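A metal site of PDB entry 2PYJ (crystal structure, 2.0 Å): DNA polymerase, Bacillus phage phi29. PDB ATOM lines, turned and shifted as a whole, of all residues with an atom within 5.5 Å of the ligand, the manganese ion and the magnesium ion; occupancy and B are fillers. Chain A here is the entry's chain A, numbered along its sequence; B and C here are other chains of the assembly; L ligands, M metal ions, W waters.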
ATOM      1  N   ASP A 249      27.591  21.868   1.107  1.00  0.00           N
ATOM      2  CA  ASP A 249      27.494  22.191  -0.335  1.00  0.00           C
ATOM      3  C   ASP A 249      28.800  22.829  -0.779  1.00  0.00           C
ATOM      4  O   ASP A 249      29.249  23.795  -0.181  1.00  0.00           O
ATOM      5  CB  ASP A 249      26.327  23.188  -0.569  1.00  0.00           C
ATOM      6  CG  ASP A 249      26.020  23.421  -2.071  1.00  0.00           C
ATOM      7  OD1 ASP A 249      24.952  22.928  -2.498  1.00  0.00           O
ATOM      8  OD2 ASP A 249      26.816  24.097  -2.819  1.00  0.00           O
ATOM      9  N   VAL A 250      29.407  22.289  -1.837  1.00  0.00           N
ATOM     10  CA  VAL A 250      30.674  22.845  -2.319  1.00  0.00           C
ATOM     11  C   VAL A 250      30.486  24.286  -2.834  1.00  0.00           C
ATOM     12  O   VAL A 250      29.504  24.608  -3.576  1.00  0.00           O
ATOM     13  CB  VAL A 250      31.349  21.971  -3.408  1.00  0.00           C
ATOM     14  CG1 VAL A 250      32.671  22.638  -3.879  1.00  0.00           C
ATOM     15  CG2 VAL A 250      31.645  20.593  -2.876  1.00  0.00           C
ATOM     16  N   ASN A 251      31.405  25.160  -2.396  1.00  0.00           N
ATOM     17  CA  ASN A 251      31.513  26.509  -2.927  1.00  0.00           C
ATOM     18  C   ASN A 251      32.041  26.464  -4.356  1.00  0.00           C
ATOM     19  O   ASN A 251      33.180  26.076  -4.583  1.00  0.00           O
ATOM     20  CB  ASN A 251      32.401  27.370  -2.038  1.00  0.00           C
ATOM     21  CG  ASN A 251      31.922  27.423  -0.601  1.00  0.00           C
ATOM     22  OD1 ASN A 251      30.713  27.465  -0.331  1.00  0.00           O
ATOM     23  ND2 ASN A 251      32.865  27.402   0.343  1.00  0.00           N
ATOM     24  N   SER A 252      31.186  26.813  -5.321  1.00  0.00           N
ATOM     25  CA  SER A 252      31.538  26.809  -6.758  1.00  0.00           C
ATOM     26  C   SER A 252      32.200  25.510  -7.225  1.00  0.00           C
ATOM     27  O   SER A 252      33.380  25.524  -7.599  1.00  0.00           O
ATOM     28  CB  SER A 252      32.463  27.998  -7.096  1.00  0.00           C
ATOM     29  OG  SER A 252      31.792  29.235  -6.948  1.00  0.00           O
ATOM     30  N   LEU A 253      31.452  24.400  -7.214  1.00  0.00           N
ATOM     31  CA  LEU A 253      32.045  23.082  -7.490  1.00  0.00           C
ATOM     32  C   LEU A 253      32.687  22.938  -8.871  1.00  0.00           C
ATOM     33  O   LEU A 253      33.826  22.527  -8.983  1.00  0.00           O
ATOM     34  CB  LEU A 253      31.070  21.910  -7.258  1.00  0.00           C
ATOM     35  CG  LEU A 253      31.720  20.524  -7.507  1.00  0.00           C
ATOM     36  CD1 LEU A 253      32.863  20.211  -6.520  1.00  0.00           C
ATOM     37  CD2 LEU A 253      30.707  19.370  -7.516  1.00  0.00           C
ATOM     38  N   TYR A 254      31.950  23.258  -9.927  1.00  0.00           N
ATOM     39  CA  TYR A 254      32.486  23.062 -11.280  1.00  0.00           C
ATOM     40  C   TYR A 254      33.699  23.988 -11.542  1.00  0.00           C
ATOM     41  O   TYR A 254      34.699  23.531 -12.067  1.00  0.00           O
ATOM     42  CB  TYR A 254      31.408  23.230 -12.356  1.00  0.00           C
ATOM     43  CG  TYR A 254      30.380  22.098 -12.463  1.00  0.00           C
ATOM     44  CD1 TYR A 254      29.693  21.890 -13.650  1.00  0.00           C
ATOM     45  CD2 TYR A 254      30.098  21.262 -11.370  1.00  0.00           C
ATOM     46  CE1 TYR A 254      28.728  20.871 -13.770  1.00  0.00           C
ATOM     47  CE2 TYR A 254      29.133  20.237 -11.477  1.00  0.00           C
ATOM     48  CZ  TYR A 254      28.447  20.063 -12.687  1.00  0.00           C
ATOM     49  OH  TYR A 254      27.509  19.056 -12.819  1.00  0.00           O
ATOM     50  N   PRO A 255      33.597  25.297 -11.192  1.00  0.00           N
ATOM     51  CA  PRO A 255      34.766  26.186 -11.264  1.00  0.00           C
ATOM     52  C   PRO A 255      35.977  25.728 -10.413  1.00  0.00           C
ATOM     53  O   PRO A 255      37.101  25.992 -10.790  1.00  0.00           O
ATOM     54  CB  PRO A 255      34.230  27.527 -10.730  1.00  0.00           C
ATOM     55  CG  PRO A 255      32.767  27.471 -10.987  1.00  0.00           C
ATOM     56  CD  PRO A 255      32.378  26.043 -10.781  1.00  0.00           C
ATOM     57  N   LYS A 371      32.631  37.140  -6.275  1.00  0.00           N
ATOM     58  CA  LYS A 371      31.664  36.266  -5.579  1.00  0.00           C
ATOM     59  C   LYS A 371      31.824  36.265  -4.043  1.00  0.00           C
ATOM     60  O   LYS A 371      30.828  36.335  -3.311  1.00  0.00           O
ATOM     61  CB  LYS A 371      31.765  34.834  -6.121  1.00  0.00           C
ATOM     62  CG  LYS A 371      30.699  33.881  -5.591  1.00  0.00           C
ATOM     63  CD  LYS A 371      30.730  32.578  -6.358  1.00  0.00           C
ATOM     64  CE  LYS A 371      29.819  31.532  -5.749  1.00  0.00           C
ATOM     65  NZ  LYS A 371      30.507  30.688  -4.743  1.00  0.00           N
ATOM     66  N   LYS A 383      28.826  34.250  -9.638  1.00  0.00           N
ATOM     67  CA  LYS A 383      28.582  32.806  -9.701  1.00  0.00           C
ATOM     68  C   LYS A 383      28.199  32.355 -11.125  1.00  0.00           C
ATOM     69  O   LYS A 383      28.705  31.344 -11.625  1.00  0.00           O
ATOM     70  CB  LYS A 383      27.482  32.413  -8.704  1.00  0.00           C
ATOM     71  CG  LYS A 383      26.956  30.979  -8.831  1.00  0.00           C
ATOM     72  CD  LYS A 383      26.043  30.657  -7.679  1.00  0.00           C
ATOM     73  CE  LYS A 383      25.286  29.370  -7.894  1.00  0.00           C
ATOM     74  NZ  LYS A 383      24.660  28.904  -6.609  1.00  0.00           N
ATOM     75  N   LEU A 384      27.316  33.131 -11.766  1.00  0.00           N
ATOM     76  CA  LEU A 384      26.887  32.839 -13.119  1.00  0.00           C
ATOM     77  C   LEU A 384      28.024  33.006 -14.147  1.00  0.00           C
ATOM     78  O   LEU A 384      28.093  32.222 -15.092  1.00  0.00           O
ATOM     79  CB  LEU A 384      25.671  33.722 -13.491  1.00  0.00           C
ATOM     80  CG  LEU A 384      25.032  33.569 -14.882  1.00  0.00           C
ATOM     81  CD1 LEU A 384      24.621  32.143 -15.177  1.00  0.00           C
ATOM     82  CD2 LEU A 384      23.841  34.526 -15.024  1.00  0.00           C
ATOM     83  N   ASN A 387      29.977  29.739 -13.761  1.00  0.00           N
ATOM     84  CA  ASN A 387      29.250  28.559 -14.224  1.00  0.00           C
ATOM     85  C   ASN A 387      28.916  28.555 -15.720  1.00  0.00           C
ATOM     86  O   ASN A 387      28.909  27.499 -16.358  1.00  0.00           O
ATOM     87  CB  ASN A 387      27.978  28.352 -13.387  1.00  0.00           C
ATOM     88  CG  ASN A 387      28.288  27.950 -11.958  1.00  0.00           C
ATOM     89  OD1 ASN A 387      29.349  27.392 -11.672  1.00  0.00           O
ATOM     90  ND2 ASN A 387      27.363  28.223 -11.047  1.00  0.00           N
ATOM     91  N   SER A 388      28.650  29.739 -16.284  1.00  0.00           N
ATOM     92  CA  SER A 388      28.300  29.854 -17.706  1.00  0.00           C
ATOM     93  C   SER A 388      29.508  29.683 -18.617  1.00  0.00           C
ATOM     94  O   SER A 388      29.357  29.341 -19.777  1.00  0.00           O
ATOM     95  CB  SER A 388      27.567  31.164 -18.014  1.00  0.00           C
ATOM     96  OG  SER A 388      28.398  32.292 -17.857  1.00  0.00           O
ATOM     97  N   TYR A 390      31.819  27.319 -18.057  1.00  0.00           N
ATOM     98  CA  TYR A 390      31.710  25.872 -18.209  1.00  0.00           C
ATOM     99  C   TYR A 390      30.670  25.539 -19.292  1.00  0.00           C
ATOM    100  O   TYR A 390      30.960  24.807 -20.256  1.00  0.00           O
ATOM    101  CB  TYR A 390      31.349  25.184 -16.874  1.00  0.00           C
ATOM    102  CG  TYR A 390      30.407  24.006 -17.056  1.00  0.00           C
ATOM    103  CD1 TYR A 390      30.796  22.881 -17.799  1.00  0.00           C
ATOM    104  CD2 TYR A 390      29.127  24.018 -16.506  1.00  0.00           C
ATOM    105  CE1 TYR A 390      29.956  21.829 -17.975  1.00  0.00           C
ATOM    106  CE2 TYR A 390      28.257  22.938 -16.685  1.00  0.00           C
ATOM    107  CZ  TYR A 390      28.681  21.854 -17.427  1.00  0.00           C
ATOM    108  OH  TYR A 390      27.829  20.796 -17.620  1.00  0.00           O
ATOM    109  N   GLY A 391      29.470  26.087 -19.142  1.00  0.00           N
ATOM    110  CA  GLY A 391      28.370  25.832 -20.066  1.00  0.00           C
ATOM    111  C   GLY A 391      28.715  26.154 -21.496  1.00  0.00           C
ATOM    112  O   GLY A 391      28.364  25.391 -22.412  1.00  0.00           O
ATOM    113  N   ASP A 456      22.802  16.142  -4.439  1.00  0.00           N
ATOM    114  CA  ASP A 456      22.468  16.757  -5.733  1.00  0.00           C
ATOM    115  C   ASP A 456      23.636  17.572  -6.257  1.00  0.00           C
ATOM    116  O   ASP A 456      23.799  18.736  -5.899  1.00  0.00           O
ATOM    117  CB  ASP A 456      21.183  17.605  -5.678  1.00  0.00           C
ATOM    118  CG  ASP A 456      20.688  17.988  -7.089  1.00  0.00           C
ATOM    119  OD1 ASP A 456      21.454  17.825  -8.071  1.00  0.00           O
ATOM    120  OD2 ASP A 456      19.532  18.449  -7.203  1.00  0.00           O
ATOM    121  N   THR A 457      24.439  16.922  -7.089  1.00  0.00           N
ATOM    122  CA  THR A 457      25.511  17.564  -7.863  1.00  0.00           C
ATOM    123  C   THR A 457      26.766  17.860  -7.039  1.00  0.00           C
ATOM    124  O   THR A 457      27.851  17.415  -7.384  1.00  0.00           O
ATOM    125  CB  THR A 457      25.016  18.834  -8.622  1.00  0.00           C
ATOM    126  OG1 THR A 457      23.865  18.492  -9.419  1.00  0.00           O
ATOM    127  CG2 THR A 457      26.103  19.403  -9.518  1.00  0.00           C
ATOM    128  N   ASP A 458      26.595  18.621  -5.958  1.00  0.00           N
ATOM    129  CA  ASP A 458      27.723  19.105  -5.161  1.00  0.00           C
ATOM    130  C   ASP A 458      27.366  19.222  -3.678  1.00  0.00           C
ATOM    131  O   ASP A 458      27.966  20.005  -2.957  1.00  0.00           O
ATOM    132  CB  ASP A 458      28.244  20.460  -5.708  1.00  0.00           C
ATOM    133  CG  ASP A 458      27.352  21.634  -5.334  1.00  0.00           C
ATOM    134  OD1 ASP A 458      27.863  22.796  -5.148  1.00  0.00           O
ATOM    135  OD2 ASP A 458      26.129  21.406  -5.217  1.00  0.00           O
ATOM    136  N   SER A 459      26.380  18.448  -3.240  1.00  0.00           N
ATOM    137  CA  SER A 459      25.951  18.485  -1.860  1.00  0.00           C
ATOM    138  C   SER A 459      25.929  17.092  -1.269  1.00  0.00           C
ATOM    139  O   SER A 459      25.765  16.107  -1.989  1.00  0.00           O
ATOM    140  CB  SER A 459      24.552  19.116  -1.745  1.00  0.00           C
ATOM    141  OG  SER A 459      23.571  18.295  -2.343  1.00  0.00           O
ATOM    142  N   GLU A 486      25.860  24.214   4.890  1.00  0.00           N
ATOM    143  CA  GLU A 486      24.697  24.918   4.374  1.00  0.00           C
ATOM    144  C   GLU A 486      23.602  25.047   5.423  1.00  0.00           C
ATOM    145  O   GLU A 486      23.016  26.124   5.591  1.00  0.00           O
ATOM    146  CB  GLU A 486      24.150  24.222   3.133  1.00  0.00           C
ATOM    147  CG  GLU A 486      22.876  24.846   2.586  1.00  0.00           C
ATOM    148  CD  GLU A 486      22.249  24.023   1.494  1.00  0.00           C
ATOM    149  OE1 GLU A 486      22.862  23.920   0.409  1.00  0.00           O
ATOM    150  OE2 GLU A 486      21.144  23.471   1.724  1.00  0.00           O
ATOM    151  P    DC B   4      23.824  32.476 -24.405  1.00  0.00           P
ATOM    152  OP1  DC B   4      23.017  32.609 -23.175  1.00  0.00           O
ATOM    153  OP2  DC B   4      24.850  33.469 -24.733  1.00  0.00           O
ATOM    154  O5'  DC B   4      24.540  31.063 -24.521  1.00  0.00           O
ATOM    155  C5'  DC B   4      23.930  29.875 -24.124  1.00  0.00           C
ATOM    156  C4'  DC B   4      24.994  29.062 -23.434  1.00  0.00           C
ATOM    157  O4'  DC B   4      25.466  29.782 -22.256  1.00  0.00           O
ATOM    158  C3'  DC B   4      24.494  27.722 -22.952  1.00  0.00           C
ATOM    159  O3'  DC B   4      24.643  26.762 -24.010  1.00  0.00           O
ATOM    160  C2'  DC B   4      25.436  27.468 -21.791  1.00  0.00           C
ATOM    161  C1'  DC B   4      25.690  28.863 -21.210  1.00  0.00           C
ATOM    162  N1   DC B   4      24.806  29.153 -20.011  1.00  0.00           N
ATOM    163  C2   DC B   4      25.029  28.409 -18.834  1.00  0.00           C
ATOM    164  O2   DC B   4      25.919  27.559 -18.802  1.00  0.00           O
ATOM    165  N3   DC B   4      24.252  28.640 -17.764  1.00  0.00           N
ATOM    166  C4   DC B   4      23.292  29.542 -17.797  1.00  0.00           C
ATOM    167  N4   DC B   4      22.575  29.690 -16.692  1.00  0.00           N
ATOM    168  C5   DC B   4      23.032  30.321 -18.971  1.00  0.00           C
ATOM    169  C6   DC B   4      23.803  30.092 -20.048  1.00  0.00           C
ATOM    170  P    DG B   5      23.625  25.525 -24.153  1.00  0.00           P
ATOM    171  OP1  DG B   5      24.015  24.821 -25.401  1.00  0.00           O
ATOM    172  OP2  DG B   5      22.269  26.038 -23.916  1.00  0.00           O
ATOM    173  O5'  DG B   5      23.964  24.572 -22.911  1.00  0.00           O
ATOM    174  C5'  DG B   5      25.228  23.894 -22.859  1.00  0.00           C
ATOM    175  C4'  DG B   5      25.341  23.103 -21.572  1.00  0.00           C
ATOM    176  O4'  DG B   5      25.388  24.016 -20.440  1.00  0.00           O
ATOM    177  C3'  DG B   5      24.138  22.226 -21.264  1.00  0.00           C
ATOM    178  O3'  DG B   5      24.224  21.028 -22.008  1.00  0.00           O
ATOM    179  C2'  DG B   5      24.331  22.014 -19.768  1.00  0.00           C
ATOM    180  C1'  DG B   5      24.847  23.360 -19.306  1.00  0.00           C
ATOM    181  N9   DG B   5      23.841  24.210 -18.655  1.00  0.00           N
ATOM    182  C8   DG B   5      23.121  25.271 -19.170  1.00  0.00           C
ATOM    183  N7   DG B   5      22.297  25.814 -18.293  1.00  0.00           N
ATOM    184  C5   DG B   5      22.492  25.040 -17.137  1.00  0.00           C
ATOM    185  C6   DG B   5      21.898  25.118 -15.853  1.00  0.00           C
ATOM    186  O6   DG B   5      21.043  25.926 -15.483  1.00  0.00           O
ATOM    187  N1   DG B   5      22.380  24.140 -14.954  1.00  0.00           N
ATOM    188  C2   DG B   5      23.329  23.188 -15.265  1.00  0.00           C
ATOM    189  N2   DG B   5      23.704  22.322 -14.297  1.00  0.00           N
ATOM    190  N3   DG B   5      23.890  23.108 -16.469  1.00  0.00           N
ATOM    191  C4   DG B   5      23.428  24.053 -17.338  1.00  0.00           C
ATOM    192  N1  DOC C  10      21.272  23.155 -10.196  1.00  0.00           N
ATOM    193  C2  DOC C  10      21.681  23.204 -11.550  1.00  0.00           C
ATOM    194  N3  DOC C  10      21.358  24.283 -12.300  1.00  0.00           N
ATOM    195  C4  DOC C  10      20.665  25.321 -11.784  1.00  0.00           C
ATOM    196  C5  DOC C  10      20.258  25.298 -10.458  1.00  0.00           C
ATOM    197  C6  DOC C  10      20.579  24.187  -9.667  1.00  0.00           C
ATOM    198  O2  DOC C  10      22.318  22.255 -12.044  1.00  0.00           O
ATOM    199  N4  DOC C  10      20.365  26.366 -12.568  1.00  0.00           N
ATOM    200  C1' DOC C  10      21.641  21.959  -9.418  1.00  0.00           C
ATOM    201  C2' DOC C  10      23.104  22.076  -8.984  1.00  0.00           C
ATOM    202  C3' DOC C  10      23.051  22.260  -7.487  1.00  0.00           C
ATOM    203  C4' DOC C  10      21.711  21.686  -7.096  1.00  0.00           C
ATOM    204  O4' DOC C  10      20.847  21.849  -8.243  1.00  0.00           O
ATOM    205  C5' DOC C  10      21.124  22.405  -5.882  1.00  0.00           C
ATOM    206  O5' DOC C  10      20.496  21.392  -5.110  1.00  0.00           O
ATOM    207  P   DOC C  10      18.988  21.548  -4.548  1.00  0.00           P
ATOM    208  OP1 DOC C  10      18.836  20.464  -3.534  1.00  0.00           O
ATOM    209  OP2 DOC C  10      18.820  22.975  -4.098  1.00  0.00           O
HETATM  210  P1  LIG L   1      27.733  27.972  -4.485  1.00  0.00           P
HETATM  211  O1  LIG L   1      26.600  28.940  -4.689  1.00  0.00           O
HETATM  212  O2  LIG L   1      28.875  28.596  -3.733  1.00  0.00           O
HETATM  213  O3  LIG L   1      27.409  26.507  -4.058  1.00  0.00           O
HETATM  214  O4  LIG L   1      28.268  27.815  -6.008  1.00  0.00           O
HETATM  215  P2  LIG L   1      28.065  26.526  -6.964  1.00  0.00           P
HETATM  216  O5  LIG L   1      28.688  26.881  -8.302  1.00  0.00           O
HETATM  217  O6  LIG L   1      28.383  25.232  -6.198  1.00  0.00           O
HETATM  218  O7  LIG L   1      26.468  26.524  -7.257  1.00  0.00           O
HETATM  219  P3  LIG L   1      25.470  25.327  -6.872  1.00  0.00           P
HETATM  220  O8  LIG L   1      24.066  25.955  -6.961  1.00  0.00           O
HETATM  221  O9  LIG L   1      25.936  24.577  -5.587  1.00  0.00           O
HETATM  222  O10 LIG L   1      25.554  24.410  -8.163  1.00  0.00           O
HETATM  223  C1  LIG L   1      26.481  23.350  -8.266  1.00  0.00           C
HETATM  224  C2  LIG L   1      26.985  23.246  -9.682  1.00  0.00           C
HETATM  225  O11 LIG L   1      25.906  22.996 -10.628  1.00  0.00           O
HETATM  226  C3  LIG L   1      27.713  24.477 -10.199  1.00  0.00           C
HETATM  227  O12 LIG L   1      29.073  24.599  -9.756  1.00  0.00           O
HETATM  228  C4  LIG L   1      27.635  24.233 -11.685  1.00  0.00           C
HETATM  229  C5  LIG L   1      26.231  23.630 -11.845  1.00  0.00           C
HETATM  230  N1  LIG L   1      25.360  24.794 -12.066  1.00  0.00           N
HETATM  231  C6  LIG L   1      24.595  25.455 -11.167  1.00  0.00           C
HETATM  232  N2  LIG L   1      23.989  26.511 -11.778  1.00  0.00           N
HETATM  233  C7  LIG L   1      24.376  26.517 -13.056  1.00  0.00           C
HETATM  234  C8  LIG L   1      24.121  27.343 -14.254  1.00  0.00           C
HETATM  235  O13 LIG L   1      23.358  28.326 -14.215  1.00  0.00           O
HETATM  236  N3  LIG L   1      24.732  27.024 -15.387  1.00  0.00           N
HETATM  237  C9  LIG L   1      25.572  25.969 -15.497  1.00  0.00           C
HETATM  238  N4  LIG L   1      26.138  25.739 -16.695  1.00  0.00           N
HETATM  239  N5  LIG L   1      25.858  25.160 -14.435  1.00  0.00           N
HETATM  240  C10 LIG L   1      25.290  25.399 -13.232  1.00  0.00           C
HETATM  241 MN    MN M   1      27.657  24.620  -4.506  1.00  0.00          MN
HETATM  242 MG    MG M   2      24.707  22.939  -4.629  1.00  0.00          MG
HETATM  243  O   HOH W   1      23.410  21.216  -4.201  1.00  0.00           O
HETATM  244  O   HOH W   2      24.644  26.468  -3.094  1.00  0.00           O
HETATM  245  O   HOH W   3      22.502  28.304 -10.175  1.00  0.00           O
HETATM  246  O   HOH W   4      25.134  30.046 -11.926  1.00  0.00           O
HETATM  247  O   HOH W   5      21.432  25.536  -6.571  1.00  0.00           O
HETATM  248  O   HOH W   6      27.981  30.752  -1.256  1.00  0.00           O
HETATM  249  O   HOH W   7      28.329  26.501  -1.120  1.00  0.00           O
HETATM  250  O   HOH W   8      22.810  25.047  -4.396  1.00  0.00           O
HETATM  251  O   HOH W   9      26.925  31.461  -3.974  1.00  0.00           O
HETATM  252  O   HOH W  10      30.099  29.129  -9.020  1.00  0.00           O
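Water W1 lies within hydrogen-bond range of O of Asp 456 (3.0 Å), O5' of DOC 10 of chain C (3.1 Å) and OG of Ser 459 (3.5 Å). Water W10 lies within hydrogen-bond range of the side-chain hydroxyl (OG) of Ser 252 (2.7 Å), an oxygen (O5) of the ligand (2.7 Å) and the side-chain amide oxygen (OD1) of Asn 387 (3.3 Å). Water W7 lies within hydrogen-bond range of OD1 of Asn 251 (2.7 Å), O of Asp 249 (3.0 Å) and O2 of the ligand (3.4 Å). Water W4 lies within hydrogen-bond range of ND2 of Asn 387 (3.0 Å) and O13 of the ligand (3.4 Å).
Residues that only touch the magnesium ion: DOC 10 of chain C (3.4 Å). Within 4 Å of the magnesium ion: Asp 249, Asp 458 and DOC 10 of chain C. Along chain A the residues within 4 Å of the magnesium ion span positions 249 to 458. The nearest printed residue that does not touch the magnesium ion is Asp 456 (4.5 Å).
The magnesium ion is bound by OD1 of Asp 249 (2.1 Å), OD2 of Asp 458 (2.2 Å), water W1 (2.2 Å) and O9 of the ligand (2.3 Å). The magnesium ion has four donor atoms within binding distance. Slightly farther from the magnesium ion lies water W8 (2.8 Å).
The side-chain amide nitrogen (ND2) of Asn 387 lies close to the backbone carbonyl oxygen (O) of Lys 383 (3.4 Å). OD1 of Asp 456 sits at hydrogen-bond distance from OG1 of Thr 457 (2.8 Å). N2 of DG 5 of chain B lies close to O2 of DOC 10 of chain C, 2.6 Å away. NZ of Lys 371 lies within hydrogen-bond range of OG of Ser 252.
N3 of DOC 10 of chain C sits close to N2 of the ligand (3.5 Å). Asn 251 touches the ligand. CD of Pro 255 touches O12 of the ligand (3.7 Å). CD2 of Tyr 390 touches N4 of the ligand, 3.5 Å away. Thr 457 touches the ligand. Hydrophobic or aromatic side chains within 4 Å of the ligand: Tyr 254, Pro 255 and Tyr 390. Of the 22 residues printed, 16 come within 4 Å of the ligand.
The backbone NH (N) of Tyr 254 sits at hydrogen-bond distance from an oxygen (O12) of the ligand. N9 of DG 5 of chain B sits close to N4 of the ligand (3.4 Å). A nitrogen (N4) of the ligand sits at hydrogen-bond distance from O2 of DC 4 of chain B. N of Ser 252 lies within hydrogen-bond range of O4 of the ligand, at 3.2 Å. O5 of the ligand is in hydrogen-bond range of ND2 of Asn 387, at 3.3 Å. NZ of Lys 383 is in salt-bridge range of O1 of the ligand. An oxygen (O2) of the ligand lies within salt-bridge range of the side-chain amino group (NZ) of Lys 371 (2.8 Å). The backbone carbonyl oxygen (O) of Asn 387 is in hydrogen-bond range of a nitrogen (N4) of the ligand (3.3 Å). N of Leu 253 lies within hydrogen-bond range of O12 of the ligand, 3.5 Å away.
The manganese ion is bound by an oxygen (O6) of the ligand, the side-chain carboxylate of Asp 458, an oxygen (O3) of the ligand, the side-chain carboxylate of Asp 249, an oxygen (O9) of the ligand and the backbone carbonyl oxygen of Val 250.
Three residues have an atom within 4 Å of the manganese ion: Asp 249, Val 250 and Asp 458.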
